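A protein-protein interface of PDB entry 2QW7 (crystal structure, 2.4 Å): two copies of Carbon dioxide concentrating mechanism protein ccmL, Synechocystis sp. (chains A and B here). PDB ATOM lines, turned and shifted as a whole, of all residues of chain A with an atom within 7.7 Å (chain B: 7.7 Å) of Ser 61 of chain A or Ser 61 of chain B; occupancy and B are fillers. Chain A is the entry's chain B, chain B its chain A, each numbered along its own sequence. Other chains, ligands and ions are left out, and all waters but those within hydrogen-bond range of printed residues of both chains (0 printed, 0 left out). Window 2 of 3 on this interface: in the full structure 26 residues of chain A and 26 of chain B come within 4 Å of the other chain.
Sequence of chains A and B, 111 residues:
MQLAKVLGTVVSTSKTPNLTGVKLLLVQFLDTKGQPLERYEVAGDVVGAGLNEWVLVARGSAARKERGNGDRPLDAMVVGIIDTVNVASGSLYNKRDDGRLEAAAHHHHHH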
ATOM      1  N   ALA A  58     -27.972 -28.294  29.841  1.00  0.00           N
ATOM      2  CA  ALA A  58     -27.707 -27.549  28.615  1.00  0.00           C
ATOM      3  C   ALA A  58     -27.149 -26.105  28.900  1.00  0.00           C
ATOM      4  O   ALA A  58     -27.695 -25.363  29.703  1.00  0.00           O
ATOM      5  CB  ALA A  58     -28.968 -27.490  27.812  1.00  0.00           C
ATOM      6  N   ARG A  59     -26.078 -25.689  28.240  1.00  0.00           N
ATOM      7  CA  ARG A  59     -25.508 -24.353  28.507  1.00  0.00           C
ATOM      8  C   ARG A  59     -25.621 -23.381  27.360  1.00  0.00           C
ATOM      9  O   ARG A  59     -25.943 -23.719  26.210  1.00  0.00           O
ATOM     10  CB  ARG A  59     -24.035 -24.431  29.030  1.00  0.00           C
ATOM     11  CG  ARG A  59     -23.986 -25.498  30.071  1.00  0.00           C
ATOM     12  CD  ARG A  59     -22.725 -25.832  30.649  1.00  0.00           C
ATOM     13  NE  ARG A  59     -21.548 -26.093  29.829  1.00  0.00           N
ATOM     14  CZ  ARG A  59     -21.348 -27.101  28.979  1.00  0.00           C
ATOM     15  NH1 ARG A  59     -22.300 -27.942  28.601  1.00  0.00           N
ATOM     16  NH2 ARG A  59     -20.137 -27.193  28.425  1.00  0.00           N
ATOM     17  N   GLY A  60     -25.466 -22.111  27.687  1.00  0.00           N
ATOM     18  CA  GLY A  60     -25.551 -21.101  26.622  1.00  0.00           C
ATOM     19  C   GLY A  60     -26.983 -20.975  26.145  1.00  0.00           C
ATOM     20  O   GLY A  60     -27.920 -21.254  26.859  1.00  0.00           O
ATOM     21  N   SER A  61     -27.112 -20.527  24.914  1.00  0.00           N
ATOM     22  CA  SER A  61     -28.352 -20.318  24.229  1.00  0.00           C
ATOM     23  C   SER A  61     -29.264 -21.528  24.079  1.00  0.00           C
ATOM     24  O   SER A  61     -30.394 -21.377  23.685  1.00  0.00           O
ATOM     25  CB  SER A  61     -28.035 -19.727  22.845  1.00  0.00           C
ATOM     26  OG  SER A  61     -27.160 -20.456  21.976  1.00  0.00           O
ATOM     27  N   ALA A  62     -28.724 -22.720  24.327  1.00  0.00           N
ATOM     28  CA  ALA A  62     -29.427 -24.000  24.236  1.00  0.00           C
ATOM     29  C   ALA A  62     -30.499 -23.974  25.310  1.00  0.00           C
ATOM     30  O   ALA A  62     -31.609 -24.506  25.168  1.00  0.00           O
ATOM     31  CB  ALA A  62     -28.441 -25.113  24.535  1.00  0.00           C
ATOM     32  N   ALA A  63     -30.112 -23.368  26.438  1.00  0.00           N
ATOM     33  CA  ALA A  63     -30.973 -23.288  27.621  1.00  0.00           C
ATOM     34  C   ALA A  63     -32.242 -22.489  27.341  1.00  0.00           C
ATOM     35  O   ALA A  63     -33.127 -22.426  28.189  1.00  0.00           O
ATOM     36  CB  ALA A  63     -30.226 -22.719  28.868  1.00  0.00           C
ATOM     37  N   ARG A  64     -32.331 -21.847  26.193  1.00  0.00           N
ATOM     38  CA  ARG A  64     -33.551 -21.071  25.879  1.00  0.00           C
ATOM     39  C   ARG A  64     -34.340 -21.677  24.750  1.00  0.00           C
ATOM     40  O   ARG A  64     -35.165 -21.025  24.139  1.00  0.00           O
ATOM     41  CB  ARG A  64     -33.229 -19.604  25.583  1.00  0.00           C
ATOM     42  CG  ARG A  64     -32.404 -18.945  26.731  1.00  0.00           C
ATOM     43  CD  ARG A  64     -32.241 -17.456  26.482  1.00  0.00           C
ATOM     44  NE  ARG A  64     -31.723 -17.179  25.138  1.00  0.00           N
ATOM     45  CZ  ARG A  64     -30.454 -17.164  24.822  1.00  0.00           C
ATOM     46  NH1 ARG A  64     -29.558 -17.462  25.774  1.00  0.00           N
ATOM     47  NH2 ARG A  64     -30.078 -16.914  23.567  1.00  0.00           N
ATOM     48  N   LYS A  65     -34.137 -22.961  24.502  1.00  0.00           N
ATOM     49  CA  LYS A  65     -34.853 -23.606  23.409  1.00  0.00           C
ATOM     50  C   LYS A  65     -36.007 -24.517  23.845  1.00  0.00           C
ATOM     51  O   LYS A  65     -36.343 -25.476  23.145  1.00  0.00           O
ATOM     52  CB  LYS A  65     -33.907 -24.265  22.405  1.00  0.00           C
ATOM     53  CG  LYS A  65     -34.323 -23.931  20.916  1.00  0.00           C
ATOM     54  CD  LYS A  65     -33.922 -22.480  20.548  1.00  0.00           C
ATOM     55  CE  LYS A  65     -34.561 -21.951  19.283  1.00  0.00           C
ATOM     56  NZ  LYS A  65     -34.702 -20.446  19.227  1.00  0.00           N
ATOM     57  N   GLU A  66     -36.650 -24.181  24.966  1.00  0.00           N
ATOM     58  CA  GLU A  66     -37.891 -24.845  25.418  1.00  0.00           C
ATOM     59  C   GLU A  66     -39.128 -24.020  25.020  1.00  0.00           C
ATOM     60  O   GLU A  66     -39.079 -22.812  24.875  1.00  0.00           O
ATOM     61  CB  GLU A  66     -37.900 -25.017  26.939  1.00  0.00           C
ATOM     62  CG  GLU A  66     -36.631 -25.675  27.522  1.00  0.00           C
ATOM     63  CD  GLU A  66     -35.610 -24.646  27.972  1.00  0.00           C
ATOM     64  OE1 GLU A  66     -35.820 -23.980  29.043  1.00  0.00           O
ATOM     65  OE2 GLU A  66     -34.621 -24.500  27.229  1.00  0.00           O
ATOM     66  N   ASN A  69     -39.322 -20.420  26.774  1.00  0.00           N
ATOM     67  CA  ASN A  69     -38.129 -19.882  27.414  1.00  0.00           C
ATOM     68  C   ASN A  69     -37.238 -19.059  26.537  1.00  0.00           C
ATOM     69  O   ASN A  69     -36.100 -18.759  26.964  1.00  0.00           O
ATOM     70  CB  ASN A  69     -37.297 -20.986  28.047  1.00  0.00           C
ATOM     71  CG  ASN A  69     -38.056 -21.727  29.074  1.00  0.00           C
ATOM     72  OD1 ASN A  69     -37.808 -21.602  30.305  1.00  0.00           O
ATOM     73  ND2 ASN A  69     -39.037 -22.483  28.597  1.00  0.00           N
ATOM     74  N   GLY A  70     -37.758 -18.693  25.368  1.00  0.00           N
ATOM     75  CA  GLY A  70     -36.976 -17.971  24.364  1.00  0.00           C
ATOM     76  C   GLY A  70     -36.503 -16.569  24.710  1.00  0.00           C
ATOM     77  O   GLY A  70     -35.425 -16.128  24.256  1.00  0.00           O
ATOM     78  N   ARG A  72     -36.198 -15.544  27.991  1.00  0.00           N
ATOM     79  CA  ARG A  72     -35.774 -15.544  29.387  1.00  0.00           C
ATOM     80  C   ARG A  72     -34.280 -15.500  29.514  1.00  0.00           C
ATOM     81  O   ARG A  72     -33.574 -16.119  28.741  1.00  0.00           O
ATOM     82  CB  ARG A  72     -36.288 -16.821  30.043  1.00  0.00           C
ATOM     83  CG  ARG A  72     -37.807 -16.996  30.024  1.00  0.00           C
ATOM     84  CD  ARG A  72     -38.197 -18.276  30.744  1.00  0.00           C
ATOM     85  NE  ARG A  72     -39.652 -18.413  30.918  1.00  0.00           N
ATOM     86  CZ  ARG A  72     -40.267 -18.326  32.096  1.00  0.00           C
ATOM     87  NH1 ARG A  72     -39.549 -18.115  33.206  1.00  0.00           N
ATOM     88  NH2 ARG A  72     -41.594 -18.460  32.160  1.00  0.00           N
ATOM     89  N   PRO A  73     -33.747 -14.836  30.530  1.00  0.00           N
ATOM     90  CA  PRO A  73     -32.275 -14.776  30.667  1.00  0.00           C
ATOM     91  C   PRO A  73     -31.585 -16.042  31.141  1.00  0.00           C
ATOM     92  O   PRO A  73     -30.717 -15.996  32.071  1.00  0.00           O
ATOM     93  CB  PRO A  73     -32.085 -13.729  31.780  1.00  0.00           C
ATOM     94  CG  PRO A  73     -33.335 -13.853  32.615  1.00  0.00           C
ATOM     95  CD  PRO A  73     -34.438 -14.075  31.592  1.00  0.00           C
ATOM     96  N   LEU A  74     -31.891 -17.174  30.512  1.00  0.00           N
ATOM     97  CA  LEU A  74     -31.252 -18.438  31.014  1.00  0.00           C
ATOM     98  C   LEU A  74     -30.025 -18.841  30.279  1.00  0.00           C
ATOM     99  O   LEU A  74     -29.957 -18.948  29.057  1.00  0.00           O
ATOM    100  CB  LEU A  74     -32.153 -19.674  31.157  1.00  0.00           C
ATOM    101  CG  LEU A  74     -33.303 -19.381  32.112  1.00  0.00           C
ATOM    102  CD1 LEU A  74     -34.627 -19.974  31.611  1.00  0.00           C
ATOM    103  CD2 LEU A  74     -32.848 -19.729  33.514  1.00  0.00           C
ATOM    104  N   ASP A  75     -29.010 -19.057  31.105  1.00  0.00           N
ATOM    105  CA  ASP A  75     -27.722 -19.491  30.591  1.00  0.00           C
ATOM    106  C   ASP A  75     -27.470 -20.988  30.805  1.00  0.00           C
ATOM    107  O   ASP A  75     -26.532 -21.534  30.194  1.00  0.00           O
ATOM    108  CB  ASP A  75     -26.588 -18.518  30.881  1.00  0.00           C
ATOM    109  CG  ASP A  75     -26.131 -18.575  32.311  1.00  0.00           C
ATOM    110  OD1 ASP A  75     -25.025 -18.043  32.614  1.00  0.00           O
ATOM    111  OD2 ASP A  75     -26.866 -19.205  33.106  1.00  0.00           O
ATOM    112  N   ALA A  76     -28.326 -21.662  31.581  1.00  0.00           N
ATOM    113  CA  ALA A  76     -28.182 -23.084  31.922  1.00  0.00           C
ATOM    114  C   ALA A  76     -29.591 -23.594  32.135  1.00  0.00           C
ATOM    115  O   ALA A  76     -30.421 -22.893  32.743  1.00  0.00           O
ATOM    116  CB  ALA A  76     -27.274 -23.271  33.267  1.00  0.00           C
ATOM    117  N   ALA B  58     -26.463 -13.884  34.637  1.00  0.00           N
ATOM    118  CA  ALA B  58     -26.704 -14.539  33.380  1.00  0.00           C
ATOM    119  C   ALA B  58     -25.564 -14.202  32.423  1.00  0.00           C
ATOM    120  O   ALA B  58     -25.266 -13.043  32.207  1.00  0.00           O
ATOM    121  CB  ALA B  58     -28.081 -14.065  32.755  1.00  0.00           C
ATOM    122  N   ARG B  59     -24.971 -15.211  31.787  1.00  0.00           N
ATOM    123  CA  ARG B  59     -23.938 -15.026  30.756  1.00  0.00           C
ATOM    124  C   ARG B  59     -24.322 -15.177  29.258  1.00  0.00           C
ATOM    125  O   ARG B  59     -25.404 -15.734  28.831  1.00  0.00           O
ATOM    126  CB  ARG B  59     -22.863 -16.032  30.961  1.00  0.00           C
ATOM    127  CG  ARG B  59     -21.713 -15.468  31.811  1.00  0.00           C
ATOM    128  CD  ARG B  59     -21.812 -15.887  33.160  1.00  0.00           C
ATOM    129  NE  ARG B  59     -21.062 -17.134  33.192  1.00  0.00           N
ATOM    130  CZ  ARG B  59     -21.527 -18.333  33.528  1.00  0.00           C
ATOM    131  NH1 ARG B  59     -22.806 -18.494  33.903  1.00  0.00           N
ATOM    132  NH2 ARG B  59     -20.649 -19.346  33.576  1.00  0.00           N
ATOM    133  N   GLY B  60     -23.429 -14.605  28.442  1.00  0.00           N
ATOM    134  CA  GLY B  60     -23.641 -14.772  27.006  1.00  0.00           C
ATOM    135  C   GLY B  60     -24.886 -14.122  26.517  1.00  0.00           C
ATOM    136  O   GLY B  60     -25.310 -13.164  27.073  1.00  0.00           O
ATOM    137  N   SER B  61     -25.460 -14.602  25.445  1.00  0.00           N
ATOM    138  CA  SER B  61     -26.681 -13.944  24.863  1.00  0.00           C
ATOM    139  C   SER B  61     -27.933 -13.860  25.766  1.00  0.00           C
ATOM    140  O   SER B  61     -28.914 -13.205  25.437  1.00  0.00           O
ATOM    141  CB  SER B  61     -27.003 -14.648  23.541  1.00  0.00           C
ATOM    142  OG  SER B  61     -27.198 -16.041  23.772  1.00  0.00           O
ATOM    143  N   ALA B  62     -27.909 -14.586  26.875  1.00  0.00           N
ATOM    144  CA  ALA B  62     -28.967 -14.551  27.872  1.00  0.00           C
ATOM    145  C   ALA B  62     -29.061 -13.145  28.477  1.00  0.00           C
ATOM    146  O   ALA B  62     -30.173 -12.621  28.737  1.00  0.00           O
ATOM    147  CB  ALA B  62     -28.691 -15.534  28.941  1.00  0.00           C
ATOM    148  N   ALA B  63     -27.895 -12.510  28.618  1.00  0.00           N
ATOM    149  CA  ALA B  63     -27.780 -11.141  29.169  1.00  0.00           C
ATOM    150  C   ALA B  63     -28.468 -10.042  28.312  1.00  0.00           C
ATOM    151  O   ALA B  63     -28.664  -8.921  28.755  1.00  0.00           O
ATOM    152  CB  ALA B  63     -26.283 -10.783  29.551  1.00  0.00           C
ATOM    153  N   ARG B  64     -28.917 -10.382  27.117  1.00  0.00           N
ATOM    154  CA  ARG B  64     -29.613  -9.420  26.252  1.00  0.00           C
ATOM    155  C   ARG B  64     -31.089  -9.700  26.130  1.00  0.00           C
ATOM    156  O   ARG B  64     -31.710  -9.182  25.210  1.00  0.00           O
ATOM    157  CB  ARG B  64     -29.052  -9.414  24.813  1.00  0.00           C
ATOM    158  CG  ARG B  64     -27.679  -8.786  24.688  1.00  0.00           C
ATOM    159  CD  ARG B  64     -27.189  -8.610  23.242  1.00  0.00           C
ATOM    160  NE  ARG B  64     -27.125  -9.843  22.464  1.00  0.00           N
ATOM    161  CZ  ARG B  64     -26.229 -10.804  22.624  1.00  0.00           C
ATOM    162  NH1 ARG B  64     -25.291 -10.771  23.615  1.00  0.00           N
ATOM    163  NH2 ARG B  64     -26.293 -11.846  21.796  1.00  0.00           N
ATOM    164  N   LYS B  65     -31.640 -10.517  27.025  1.00  0.00           N
ATOM    165  CA  LYS B  65     -33.041 -10.929  26.927  1.00  0.00           C
ATOM    166  C   LYS B  65     -34.045 -10.160  27.782  1.00  0.00           C
ATOM    167  O   LYS B  65     -35.182 -10.646  27.996  1.00  0.00           O
ATOM    168  CB  LYS B  65     -33.166 -12.453  27.064  1.00  0.00           C
ATOM    169  CG  LYS B  65     -32.675 -13.267  25.801  1.00  0.00           C
ATOM    170  CD  LYS B  65     -33.741 -13.592  24.715  1.00  0.00           C
ATOM    171  CE  LYS B  65     -34.236 -12.416  23.800  1.00  0.00           C
ATOM    172  NZ  LYS B  65     -33.460 -12.096  22.526  1.00  0.00           N
ATOM    173  N   GLU B  66     -33.685  -8.949  28.227  1.00  0.00           N
ATOM    174  CA  GLU B  66     -34.644  -8.130  28.950  1.00  0.00           C
ATOM    175  C   GLU B  66     -35.242  -7.071  28.001  1.00  0.00           C
ATOM    176  O   GLU B  66     -34.691  -6.788  26.937  1.00  0.00           O
ATOM    177  CB  GLU B  66     -34.062  -7.560  30.248  1.00  0.00           C
ATOM    178  CG  GLU B  66     -34.420  -8.392  31.498  1.00  0.00           C
ATOM    179  CD  GLU B  66     -33.561  -9.631  31.746  1.00  0.00           C
ATOM    180  OE1 GLU B  66     -34.140 -10.730  31.875  1.00  0.00           O
ATOM    181  OE2 GLU B  66     -32.314  -9.510  31.848  1.00  0.00           O
ATOM    182  N   ASN B  69     -32.826  -4.513  26.074  1.00  0.00           N
ATOM    183  CA  ASN B  69     -31.422  -4.877  25.977  1.00  0.00           C
ATOM    184  C   ASN B  69     -30.987  -5.708  24.775  1.00  0.00           C
ATOM    185  O   ASN B  69     -29.865  -6.183  24.716  1.00  0.00           O
ATOM    186  CB  ASN B  69     -31.082  -5.640  27.247  1.00  0.00           C
ATOM    187  CG  ASN B  69     -31.019  -4.747  28.396  1.00  0.00           C
ATOM    188  OD1 ASN B  69     -30.419  -3.707  28.294  1.00  0.00           O
ATOM    189  ND2 ASN B  69     -31.653  -5.097  29.483  1.00  0.00           N
ATOM    190  N   GLY B  70     -31.870  -5.895  23.811  1.00  0.00           N
ATOM    191  CA  GLY B  70     -31.586  -6.764  22.660  1.00  0.00           C
ATOM    192  C   GLY B  70     -30.524  -6.330  21.665  1.00  0.00           C
ATOM    193  O   GLY B  70     -29.994  -7.155  20.894  1.00  0.00           O
ATOM    194  N   LEU B  74     -24.112  -6.431  25.701  1.00  0.00           N
ATOM    195  CA  LEU B  74     -24.134  -7.067  26.995  1.00  0.00           C
ATOM    196  C   LEU B  74     -23.874  -8.606  26.969  1.00  0.00           C
ATOM    197  O   LEU B  74     -24.609  -9.378  26.313  1.00  0.00           O
ATOM    198  CB  LEU B  74     -25.435  -6.651  27.717  1.00  0.00           C
ATOM    199  CG  LEU B  74     -25.458  -5.273  28.409  1.00  0.00           C
ATOM    200  CD1 LEU B  74     -26.829  -4.785  28.903  1.00  0.00           C
ATOM    201  CD2 LEU B  74     -24.536  -5.346  29.679  1.00  0.00           C
ATOM    202  N   ASP B  75     -22.763  -8.945  27.643  1.00  0.00           N
ATOM    203  CA  ASP B  75     -22.205 -10.263  27.905  1.00  0.00           C
ATOM    204  C   ASP B  75     -22.734 -10.987  29.134  1.00  0.00           C
ATOM    205  O   ASP B  75     -22.811 -12.231  29.166  1.00  0.00           O
ATOM    206  CB  ASP B  75     -20.796 -10.012  28.474  1.00  0.00           C
ATOM    207  CG  ASP B  75     -19.725 -10.160  27.497  1.00  0.00           C
ATOM    208  OD1 ASP B  75     -19.853  -9.679  26.358  1.00  0.00           O
ATOM    209  OD2 ASP B  75     -18.724 -10.760  27.880  1.00  0.00           O
ATOM    210  N   ALA B  76     -22.941 -10.170  30.174  1.00  0.00           N
ATOM    211  CA  ALA B  76     -23.269 -10.565  31.529  1.00  0.00           C
ATOM    212  C   ALA B  76     -24.234  -9.580  32.146  1.00  0.00           C
ATOM    213  O   ALA B  76     -23.965  -8.386  32.164  1.00  0.00           O
ATOM    214  CB  ALA B  76     -22.014 -10.660  32.404  1.00  0.00           C
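OD1 of Asp 75 of chain A is in salt-bridge range of NH1 of Arg 59 of chain B (2.6 Å).
The side-chain hydroxyl of Ser 61 of chain B sits at hydrogen-bond distance from the guanidinium group of Arg 64 of chain A (3.0 Å).
The guanidinium group (NH1) of Arg 64 of chain A sits close to the backbone NH (N) of Ala 62 of chain B (3.5 Å).
N of Gly 60 of chain A sits at hydrogen-bond distance from O of Asp 75 of chain A (2.8 Å).
Among the printed residues, pairs that only touch across the chains: Ser 61 of chain A with Ser 61 of chain B (3.9 Å), Gly 70 of chain A with Lys 65 of chain B (3.1 Å), Pro 73 of chain A with Ala 58 of chain B (3.3 Å), Pro 73 of chain A with Ala 62 of chain B (3.6 Å), Pro 73 of chain A with Glu 66 of chain B (3.3 Å), Leu 74 of chain A with Ala 62 of chain B (3.6 Å) and Asp 75 of chain A with Ala 58 of chain B (3.9 Å).
No residue of chain B comes within 4 Å of Gly 60 of chain A.
Of chain B, only Ser 61 (3.9 Å) comes within 4 Å of Ser 61 of chain A.
Printed residues of chain B within 4 Å of Gly 70 of chain A: Lys 65.
Of the printed residues of chain B, Pro 73 of chain A touches Ala 58, Ala 62 and Glu 66.
Printed residues of chain B within 4 Å of Asp 75 of chain A: Ala 58 and Arg 59.
Ser 61 of chain B touches just these residues of chain A: Ser 61 and Arg 64.
Of the printed residues of chain A, Lys 65 of chain B touches Gly 70 (3.1 Å).
Asp 75 of chain B touches none of the printed residues of chain A.
The nearest residue of chain B that does not touch Ser 61 of chain A is Ala 62 of chain B (6.3 Å).
The nearest residue of chain A that does not touch Ser 61 of chain B is Gly 60 of chain A (5.5 Å).
Of the 14 printed residues of chain B, 6 touch a printed residue of chain A.
Printed residues of chain B that touch a printed residue of chain A: Ala 58, Arg 59, Ser 61, Ala 62, Lys 65 and Glu 66.
Of the 16 printed residues of chain A, 6 touch a printed residue of chain B.
Among the printed residues, 10 pairs touch across the chains.
Ser 61 of chain A touches its own counterpart, Ser 61 of chain B.
Leu 74 of chain A touches Ala 62 of chain B, but with the chains exchanged Ala 62 of chain A does not touch Leu 74 of chain B (14.1 Å).
Asp 75 of chain A touches Ala 58 of chain B, but with the chains exchanged Ala 58 of chain A does not touch Asp 75 of chain B (14.0 Å).
Asp 75 of chain A touches Arg 59 of chain B, but with the chains exchanged Arg 59 of chain A does not touch Asp 75 of chain B (11.6 Å).
14 positions are printed for both chains.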
